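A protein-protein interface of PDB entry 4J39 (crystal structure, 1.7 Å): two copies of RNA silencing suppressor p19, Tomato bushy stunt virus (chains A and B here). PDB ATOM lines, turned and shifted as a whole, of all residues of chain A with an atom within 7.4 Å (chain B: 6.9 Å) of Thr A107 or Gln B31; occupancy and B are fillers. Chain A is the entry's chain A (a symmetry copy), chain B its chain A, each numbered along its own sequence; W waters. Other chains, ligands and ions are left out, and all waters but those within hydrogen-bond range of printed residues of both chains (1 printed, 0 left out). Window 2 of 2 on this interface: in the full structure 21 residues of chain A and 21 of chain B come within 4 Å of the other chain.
The side-chain carboxylate (OD2) of Asp B32 lies within salt-bridge range of the guanidinium group (NE) of Arg B95, at 3.2 Å. O of Gly A103 sits at hydrogen-bond distance from N of Cys A88 (2.8 Å). The side-chain hydroxyl (OG1) of Thr A107 lies within hydrogen-bond range of the backbone carbonyl oxygen (O) of Gly A104 (3.0 Å). A ring nitrogen (ND1) of His A110 sits at hydrogen-bond distance from the side-chain carboxylate (OE1) of Glu A113 (3.2 Å).
Thr A107 touches two residues of chain B. Gln B31 touches just one residue of chain A: Thr A107 (3.8 Å). Printed residues of chain A within 4 Å of Arg B95: His A110. Of the printed residues of chain B, His A110 touches Arg B95 and Val B97. Of the printed residues of chain B, Gly A103 touches Gly B96 (3.7 Å). The nearest residue of chain B that does not touch Thr A107 is Arg B95 (4.7 Å). The nearest printed residue of chain A that does not touch Gln B31 is Arg A106 (6.1 Å). The nearest printed residue of chain A that does not touch Val B97 is Thr A107 (4.8 Å).
Gly B96 touches Ser A102. Val B97 touches Ser A102 (CA to O, 3.7 Å). CA of Gly A103 touches O of Gly B96 (3.7 Å). Gln B31 touches Thr A107 (NE2 to CG2, 3.8 Å). Thr A107 touches Gly B96. Arg B95 touches His A110. Val B97 touches His A110. CD2 of Leu A111 touches CB of Val B97, at 3.8 Å.
Water W1 lies within hydrogen-bond range of O of Gly B96 (2.6 Å) and N of Gly A104 (2.8 Å).
No position is printed for both chains.
Of the 15 printed residues of chain A, 5 touch a printed residue of chain B. Of the 12 printed residues of chain B, 4 touch a printed residue of chain A. Hydrophobic or aromatic side chains of chain B that line the printed part of chain A: Val B97. Along chain B the printed residues that touch a printed residue of chain A span positions 31 to 97.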
ATOM      1  N   GLN A  85       1.070  16.333 -18.391  1.00  0.00           N
ATOM      2  CA  GLN A  85       2.268  17.111 -18.746  1.00  0.00           C
ATOM      3  C   GLN A  85       2.187  17.552 -20.188  1.00  0.00           C
ATOM      4  O   GLN A  85       1.637  16.838 -21.051  1.00  0.00           O
ATOM      5  CB  GLN A  85       3.487  16.231 -18.459  1.00  0.00           C
ATOM      6  CG  GLN A  85       4.749  16.907 -18.583  1.00  0.00           C
ATOM      7  CD  GLN A  85       5.885  16.178 -17.983  1.00  0.00           C
ATOM      8  OE1 GLN A  85       6.651  16.796 -17.272  1.00  0.00           O
ATOM      9  NE2 GLN A  85       6.088  14.902 -18.337  1.00  0.00           N
ATOM     10  N   ILE A  86       2.643  18.777 -20.474  1.00  0.00           N
ATOM     11  CA  ILE A  86       2.815  19.228 -21.859  1.00  0.00           C
ATOM     12  C   ILE A  86       4.316  19.508 -22.123  1.00  0.00           C
ATOM     13  O   ILE A  86       5.076  19.665 -21.172  1.00  0.00           O
ATOM     14  CB  ILE A  86       2.045  20.557 -22.078  1.00  0.00           C
ATOM     15  CG1 ILE A  86       2.505  21.706 -21.148  1.00  0.00           C
ATOM     16  CG2 ILE A  86       0.522  20.283 -21.898  1.00  0.00           C
ATOM     17  CD1 ILE A  86       1.710  23.036 -21.332  1.00  0.00           C
ATOM     18  N   CYS A  88       7.512  21.695 -23.148  1.00  0.00           N
ATOM     19  CA  CYS A  88       7.941  23.087 -23.039  1.00  0.00           C
ATOM     20  C   CYS A  88       9.337  23.277 -23.589  1.00  0.00           C
ATOM     21  O   CYS A  88      10.130  22.351 -23.452  1.00  0.00           O
ATOM     22  CB  CYS A  88       8.072  23.536 -21.601  1.00  0.00           C
ATOM     23  SG  CYS A  88       6.484  23.449 -20.636  1.00  0.00           S
ATOM     24  N   SER A 102      14.577  21.802 -23.715  1.00  0.00           N
ATOM     25  CA  SER A 102      13.185  21.238 -23.842  1.00  0.00           C
ATOM     26  C   SER A 102      12.912  20.190 -22.772  1.00  0.00           C
ATOM     27  O   SER A 102      13.834  19.419 -22.331  1.00  0.00           O
ATOM     28  CB  SER A 102      12.969  20.633 -25.261  1.00  0.00           C
ATOM     29  OG  SER A 102      14.013  19.825 -25.684  1.00  0.00           O
ATOM     30  N   GLY A 103      11.641  20.038 -22.368  1.00  0.00           N
ATOM     31  CA  GLY A 103      11.242  18.908 -21.614  1.00  0.00           C
ATOM     32  C   GLY A 103       9.804  19.109 -21.133  1.00  0.00           C
ATOM     33  O   GLY A 103       9.157  19.998 -21.599  1.00  0.00           O
ATOM     34  N   GLY A 104       9.313  18.263 -20.241  1.00  0.00           N
ATOM     35  CA  GLY A 104       7.902  18.343 -19.827  1.00  0.00           C
ATOM     36  C   GLY A 104       7.648  19.454 -18.830  1.00  0.00           C
ATOM     37  O   GLY A 104       8.571  19.901 -18.138  1.00  0.00           O
ATOM     38  N   SER A 105       6.393  19.893 -18.701  1.00  0.00           N
ATOM     39  CA  SER A 105       6.054  20.985 -17.717  1.00  0.00           C
ATOM     40  C   SER A 105       6.435  20.691 -16.309  1.00  0.00           C
ATOM     41  O   SER A 105       6.593  21.633 -15.435  1.00  0.00           O
ATOM     42  CB  SER A 105       4.539  21.323 -17.783  1.00  0.00           C
ATOM     43  OG  SER A 105       3.703  20.210 -17.987  1.00  0.00           O
ATOM     44  N   ARG A 106       6.510  19.415 -15.967  1.00  0.00           N
ATOM     45  CA  ARG A 106       6.854  19.077 -14.590  1.00  0.00           C
ATOM     46  C   ARG A 106       8.290  19.545 -14.300  1.00  0.00           C
ATOM     47  O   ARG A 106       8.651  19.699 -13.147  1.00  0.00           O
ATOM     48  CB  ARG A 106       6.773  17.545 -14.391  1.00  0.00           C
ATOM     49  CG  ARG A 106       5.926  17.063 -13.252  1.00  0.00           C
ATOM     50  CD  ARG A 106       4.585  16.437 -13.701  1.00  0.00           C
ATOM     51  NE  ARG A 106       4.757  15.138 -14.349  1.00  0.00           N
ATOM     52  CZ  ARG A 106       3.776  14.327 -14.765  1.00  0.00           C
ATOM     53  NH1 ARG A 106       2.482  14.637 -14.596  1.00  0.00           N
ATOM     54  NH2 ARG A 106       4.127  13.185 -15.369  1.00  0.00           N
ATOM     55  N   THR A 107       9.085  19.751 -15.332  1.00  0.00           N
ATOM     56  CA  THR A 107      10.493  20.138 -15.152  1.00  0.00           C
ATOM     57  C   THR A 107      10.760  21.636 -15.405  1.00  0.00           C
ATOM     58  O   THR A 107      11.893  22.074 -15.568  1.00  0.00           O
ATOM     59  CB  THR A 107      11.486  19.278 -16.031  1.00  0.00           C
ATOM     60  OG1 THR A 107      11.453  19.787 -17.418  1.00  0.00           O
ATOM     61  CG2 THR A 107      11.128  17.814 -15.877  1.00  0.00           C
ATOM     62  N   LEU A 108       9.724  22.454 -15.488  1.00  0.00           N
ATOM     63  CA  LEU A 108       9.881  23.763 -16.015  1.00  0.00           C
ATOM     64  C   LEU A 108      10.893  24.621 -15.251  1.00  0.00           C
ATOM     65  O   LEU A 108      11.620  25.423 -15.872  1.00  0.00           O
ATOM     66  CB  LEU A 108       8.548  24.533 -16.074  1.00  0.00           C
ATOM     67  CG  LEU A 108       8.494  25.882 -16.773  1.00  0.00           C
ATOM     68  CD1 LEU A 108       8.987  25.928 -18.226  1.00  0.00           C
ATOM     69  CD2 LEU A 108       7.063  26.546 -16.652  1.00  0.00           C
ATOM     70  N   GLN A 109      10.943  24.471 -13.919  1.00  0.00           N
ATOM     71  CA  GLN A 109      11.898  25.262 -13.144  1.00  0.00           C
ATOM     72  C   GLN A 109      13.384  24.990 -13.622  1.00  0.00           C
ATOM     73  O   GLN A 109      14.180  25.930 -13.826  1.00  0.00           O
ATOM     74  CB  GLN A 109      11.703  25.025 -11.650  1.00  0.00           C
ATOM     75  CG  GLN A 109      12.550  25.974 -10.853  1.00  0.00           C
ATOM     76  CD  GLN A 109      12.200  26.030  -9.332  1.00  0.00           C
ATOM     77  OE1 GLN A 109      11.219  25.444  -8.890  1.00  0.00           O
ATOM     78  NE2 GLN A 109      13.022  26.755  -8.550  1.00  0.00           N
ATOM     79  N   HIS A 110      13.683  23.723 -13.805  1.00  0.00           N
ATOM     80  CA  HIS A 110      15.015  23.310 -14.301  1.00  0.00           C
ATOM     81  C   HIS A 110      15.179  23.729 -15.774  1.00  0.00           C
ATOM     82  O   HIS A 110      16.288  24.124 -16.175  1.00  0.00           O
ATOM     83  CB  HIS A 110      15.199  21.794 -14.176  1.00  0.00           C
ATOM     84  CG  HIS A 110      15.344  21.268 -12.784  1.00  0.00           C
ATOM     85  ND1 HIS A 110      15.908  21.986 -11.740  1.00  0.00           N
ATOM     86  CD2 HIS A 110      15.099  20.029 -12.297  1.00  0.00           C
ATOM     87  CE1 HIS A 110      15.933  21.227 -10.650  1.00  0.00           C
ATOM     88  NE2 HIS A 110      15.458  20.030 -10.969  1.00  0.00           N
ATOM     89  N   LEU A 111      14.120  23.660 -16.617  1.00  0.00           N
ATOM     90  CA  LEU A 111      14.267  24.198 -17.949  1.00  0.00           C
ATOM     91  C   LEU A 111      14.630  25.715 -17.909  1.00  0.00           C
ATOM     92  O   LEU A 111      15.496  26.145 -18.658  1.00  0.00           O
ATOM     93  CB  LEU A 111      13.042  23.972 -18.834  1.00  0.00           C
ATOM     94  CG  LEU A 111      12.548  22.578 -18.960  1.00  0.00           C
ATOM     95  CD1 LEU A 111      11.122  22.607 -19.667  1.00  0.00           C
ATOM     96  CD2 LEU A 111      13.549  21.721 -19.702  1.00  0.00           C
ATOM     97  N   CYS A 112      14.008  26.522 -17.001  1.00  0.00           N
ATOM     98  CA  CYS A 112      14.339  27.925 -16.952  1.00  0.00           C
ATOM     99  C   CYS A 112      15.808  28.170 -16.551  1.00  0.00           C
ATOM    100  O   CYS A 112      16.460  29.099 -16.993  1.00  0.00           O
ATOM    101  CB  CYS A 112      13.378  28.628 -15.906  1.00  0.00           C
ATOM    102  SG  CYS A 112      11.644  28.738 -16.722  1.00  0.00           S
ATOM    103  N   GLU A 113      16.224  27.305 -15.637  1.00  0.00           N
ATOM    104  CA  GLU A 113      17.614  27.492 -15.022  1.00  0.00           C
ATOM    105  C   GLU A 113      18.624  27.201 -16.135  1.00  0.00           C
ATOM    106  O   GLU A 113      19.569  27.947 -16.334  1.00  0.00           O
ATOM    107  CB  GLU A 113      17.826  26.521 -13.878  1.00  0.00           C
ATOM    108  CG  GLU A 113      17.231  26.962 -12.478  1.00  0.00           C
ATOM    109  CD  GLU A 113      17.050  25.746 -11.481  1.00  0.00           C
ATOM    110  OE1 GLU A 113      17.698  24.679 -11.684  1.00  0.00           O
ATOM    111  OE2 GLU A 113      16.238  25.834 -10.519  1.00  0.00           O
ATOM    112  N   THR B  27      16.248   2.386  -6.546  1.00  0.00           N
ATOM    113  CA  THR B  27      16.314   3.843  -6.279  1.00  0.00           C
ATOM    114  C   THR B  27      14.953   4.423  -5.933  1.00  0.00           C
ATOM    115  O   THR B  27      13.948   4.015  -6.511  1.00  0.00           O
ATOM    116  CB  THR B  27      16.882   4.642  -7.514  1.00  0.00           C
ATOM    117  OG1 THR B  27      15.966   4.530  -8.626  1.00  0.00           O
ATOM    118  CG2 THR B  27      18.241   4.111  -7.899  1.00  0.00           C
ATOM    119  N   ASN B  30      13.378   6.523  -9.747  1.00  0.00           N
ATOM    120  CA  ASN B  30      13.606   7.966  -9.644  1.00  0.00           C
ATOM    121  C   ASN B  30      14.337   8.588 -10.872  1.00  0.00           C
ATOM    122  O   ASN B  30      15.495   8.226 -11.158  1.00  0.00           O
ATOM    123  CB  ASN B  30      14.384   8.249  -8.360  1.00  0.00           C
ATOM    124  CG  ASN B  30      14.515   9.728  -8.061  1.00  0.00           C
ATOM    125  OD1 ASN B  30      13.853  10.574  -8.693  1.00  0.00           O
ATOM    126  ND2 ASN B  30      15.381  10.057  -7.096  1.00  0.00           N
ATOM    127  N   GLN B  31      13.656   9.538 -11.556  1.00  0.00           N
ATOM    128  CA  GLN B  31      14.187  10.302 -12.743  1.00  0.00           C
ATOM    129  C   GLN B  31      15.402  11.197 -12.433  1.00  0.00           C
ATOM    130  O   GLN B  31      16.219  11.434 -13.319  1.00  0.00           O
ATOM    131  CB  GLN B  31      13.071  11.190 -13.414  1.00  0.00           C
ATOM    132  CG  GLN B  31      13.561  12.617 -13.954  1.00  0.00           C
ATOM    133  CD  GLN B  31      12.476  13.473 -14.624  1.00  0.00           C
ATOM    134  OE1 GLN B  31      11.980  13.129 -15.707  1.00  0.00           O
ATOM    135  NE2 GLN B  31      12.130  14.607 -13.999  1.00  0.00           N
ATOM    136  N   ASP B  32      15.490  11.703 -11.200  1.00  0.00           N
ATOM    137  CA  ASP B  32      16.637  12.503 -10.766  1.00  0.00           C
ATOM    138  C   ASP B  32      17.882  11.691 -10.405  1.00  0.00           C
ATOM    139  O   ASP B  32      18.910  12.304 -10.231  1.00  0.00           O
ATOM    140  CB  ASP B  32      16.253  13.473  -9.595  1.00  0.00           C
ATOM    141  CG  ASP B  32      15.466  14.722 -10.079  1.00  0.00           C
ATOM    142  OD1 ASP B  32      14.672  15.263  -9.286  1.00  0.00           O
ATOM    143  OD2 ASP B  32      15.644  15.191 -11.237  1.00  0.00           O
ATOM    144  N   ASN B  33      17.811  10.351 -10.282  1.00  0.00           N
ATOM    145  CA  ASN B  33      19.043   9.496 -10.063  1.00  0.00           C
ATOM    146  C   ASN B  33      19.228   8.326 -11.036  1.00  0.00           C
ATOM    147  O   ASN B  33      19.293   7.190 -10.639  1.00  0.00           O
ATOM    148  CB  ASN B  33      19.238   9.090  -8.606  1.00  0.00           C
ATOM    149  CG  ASN B  33      19.731  10.286  -7.756  1.00  0.00           C
ATOM    150  OD1 ASN B  33      20.947  10.633  -7.744  1.00  0.00           O
ATOM    151  ND2 ASN B  33      18.800  10.964  -7.135  1.00  0.00           N
ATOM    152  N   PRO B  34      19.299   8.661 -12.329  1.00  0.00           N
ATOM    153  CA  PRO B  34      19.461   7.696 -13.419  1.00  0.00           C
ATOM    154  C   PRO B  34      20.849   7.101 -13.368  1.00  0.00           C
ATOM    155  O   PRO B  34      21.713   7.629 -12.692  1.00  0.00           O
ATOM    156  CB  PRO B  34      19.274   8.556 -14.634  1.00  0.00           C
ATOM    157  CG  PRO B  34      19.746   9.861 -14.320  1.00  0.00           C
ATOM    158  CD  PRO B  34      19.397  10.041 -12.822  1.00  0.00           C
ATOM    159  N   ARG B  56      27.491  11.978 -10.506  1.00  0.00           N
ATOM    160  CA  ARG B  56      27.476  13.317  -9.995  1.00  0.00           C
ATOM    161  C   ARG B  56      28.584  13.624  -9.059  1.00  0.00           C
ATOM    162  O   ARG B  56      28.438  14.512  -8.281  1.00  0.00           O
ATOM    163  CB  ARG B  56      26.148  13.607  -9.255  1.00  0.00           C
ATOM    164  CG  ARG B  56      24.883  13.494 -10.040  1.00  0.00           C
ATOM    165  CD  ARG B  56      23.905  14.378  -9.251  1.00  0.00           C
ATOM    166  NE  ARG B  56      22.516  14.049  -9.536  1.00  0.00           N
ATOM    167  CZ  ARG B  56      21.453  14.619  -8.937  1.00  0.00           C
ATOM    168  NH1 ARG B  56      21.598  15.549  -7.986  1.00  0.00           N
ATOM    169  NH2 ARG B  56      20.223  14.243  -9.300  1.00  0.00           N
ATOM    170  N   ARG B  93      20.653  14.743 -22.908  1.00  0.00           N
ATOM    171  CA  ARG B  93      19.525  14.636 -22.056  1.00  0.00           C
ATOM    172  C   ARG B  93      19.920  14.038 -20.691  1.00  0.00           C
ATOM    173  O   ARG B  93      20.625  12.989 -20.606  1.00  0.00           O
ATOM    174  CB  ARG B  93      18.447  13.795 -22.723  1.00  0.00           C
ATOM    175  CG  ARG B  93      17.318  13.521 -21.770  1.00  0.00           C
ATOM    176  CD  ARG B  93      16.054  13.384 -22.418  1.00  0.00           C
ATOM    177  NE  ARG B  93      14.953  13.171 -21.460  1.00  0.00           N
ATOM    178  CZ  ARG B  93      13.681  13.093 -21.817  1.00  0.00           C
ATOM    179  NH1 ARG B  93      13.357  13.227 -23.098  1.00  0.00           N
ATOM    180  NH2 ARG B  93      12.739  12.844 -20.924  1.00  0.00           N
ATOM    181  N   PHE B  94      19.517  14.757 -19.630  1.00  0.00           N
ATOM    182  CA  PHE B  94      19.787  14.309 -18.271  1.00  0.00           C
ATOM    183  C   PHE B  94      18.650  14.787 -17.345  1.00  0.00           C
ATOM    184  O   PHE B  94      18.272  15.975 -17.406  1.00  0.00           O
ATOM    185  CB  PHE B  94      21.143  14.860 -17.839  1.00  0.00           C
ATOM    186  CG  PHE B  94      21.583  14.385 -16.508  1.00  0.00           C
ATOM    187  CD1 PHE B  94      21.651  13.036 -16.179  1.00  0.00           C
ATOM    188  CD2 PHE B  94      21.968  15.357 -15.523  1.00  0.00           C
ATOM    189  CE1 PHE B  94      22.130  12.614 -14.896  1.00  0.00           C
ATOM    190  CE2 PHE B  94      22.366  14.944 -14.268  1.00  0.00           C
ATOM    191  CZ  PHE B  94      22.465  13.616 -13.962  1.00  0.00           C
ATOM    192  N   ARG B  95      18.058  13.872 -16.592  1.00  0.00           N
ATOM    193  CA  ARG B  95      17.067  14.264 -15.538  1.00  0.00           C
ATOM    194  C   ARG B  95      15.891  15.110 -16.099  1.00  0.00           C
ATOM    195  O   ARG B  95      15.502  16.145 -15.551  1.00  0.00           O
ATOM    196  CB  ARG B  95      17.773  15.055 -14.450  1.00  0.00           C
ATOM    197  CG  ARG B  95      18.807  14.191 -13.669  1.00  0.00           C
ATOM    198  CD  ARG B  95      19.601  15.077 -12.718  1.00  0.00           C
ATOM    199  NE  ARG B  95      18.728  15.746 -11.767  1.00  0.00           N
ATOM    200  CZ  ARG B  95      18.977  16.906 -11.152  1.00  0.00           C
ATOM    201  NH1 ARG B  95      20.118  17.601 -11.393  1.00  0.00           N
ATOM    202  NH2 ARG B  95      18.059  17.377 -10.275  1.00  0.00           N
ATOM    203  N   GLY B  96      15.351  14.677 -17.236  1.00  0.00           N
ATOM    204  CA  GLY B  96      14.166  15.290 -17.753  1.00  0.00           C
ATOM    205  C   GLY B  96      14.403  16.498 -18.668  1.00  0.00           C
ATOM    206  O   GLY B  96      13.473  17.037 -19.290  1.00  0.00           O
ATOM    207  N   VAL B  97      15.664  16.985 -18.755  1.00  0.00           N
ATOM    208  CA  VAL B  97      15.942  18.139 -19.563  1.00  0.00           C
ATOM    209  C   VAL B  97      16.912  17.804 -20.713  1.00  0.00           C
ATOM    210  O   VAL B  97      17.918  17.115 -20.487  1.00  0.00           O
ATOM    211  CB  VAL B  97      16.401  19.459 -18.770  1.00  0.00           C
ATOM    212  CG1 VAL B  97      16.195  19.493 -17.158  1.00  0.00           C
ATOM    213  CG2 VAL B  97      17.298  20.421 -19.510  1.00  0.00           C
HETATM  214  O   HOH W   1      11.005  16.156 -19.432  1.00  0.00           O
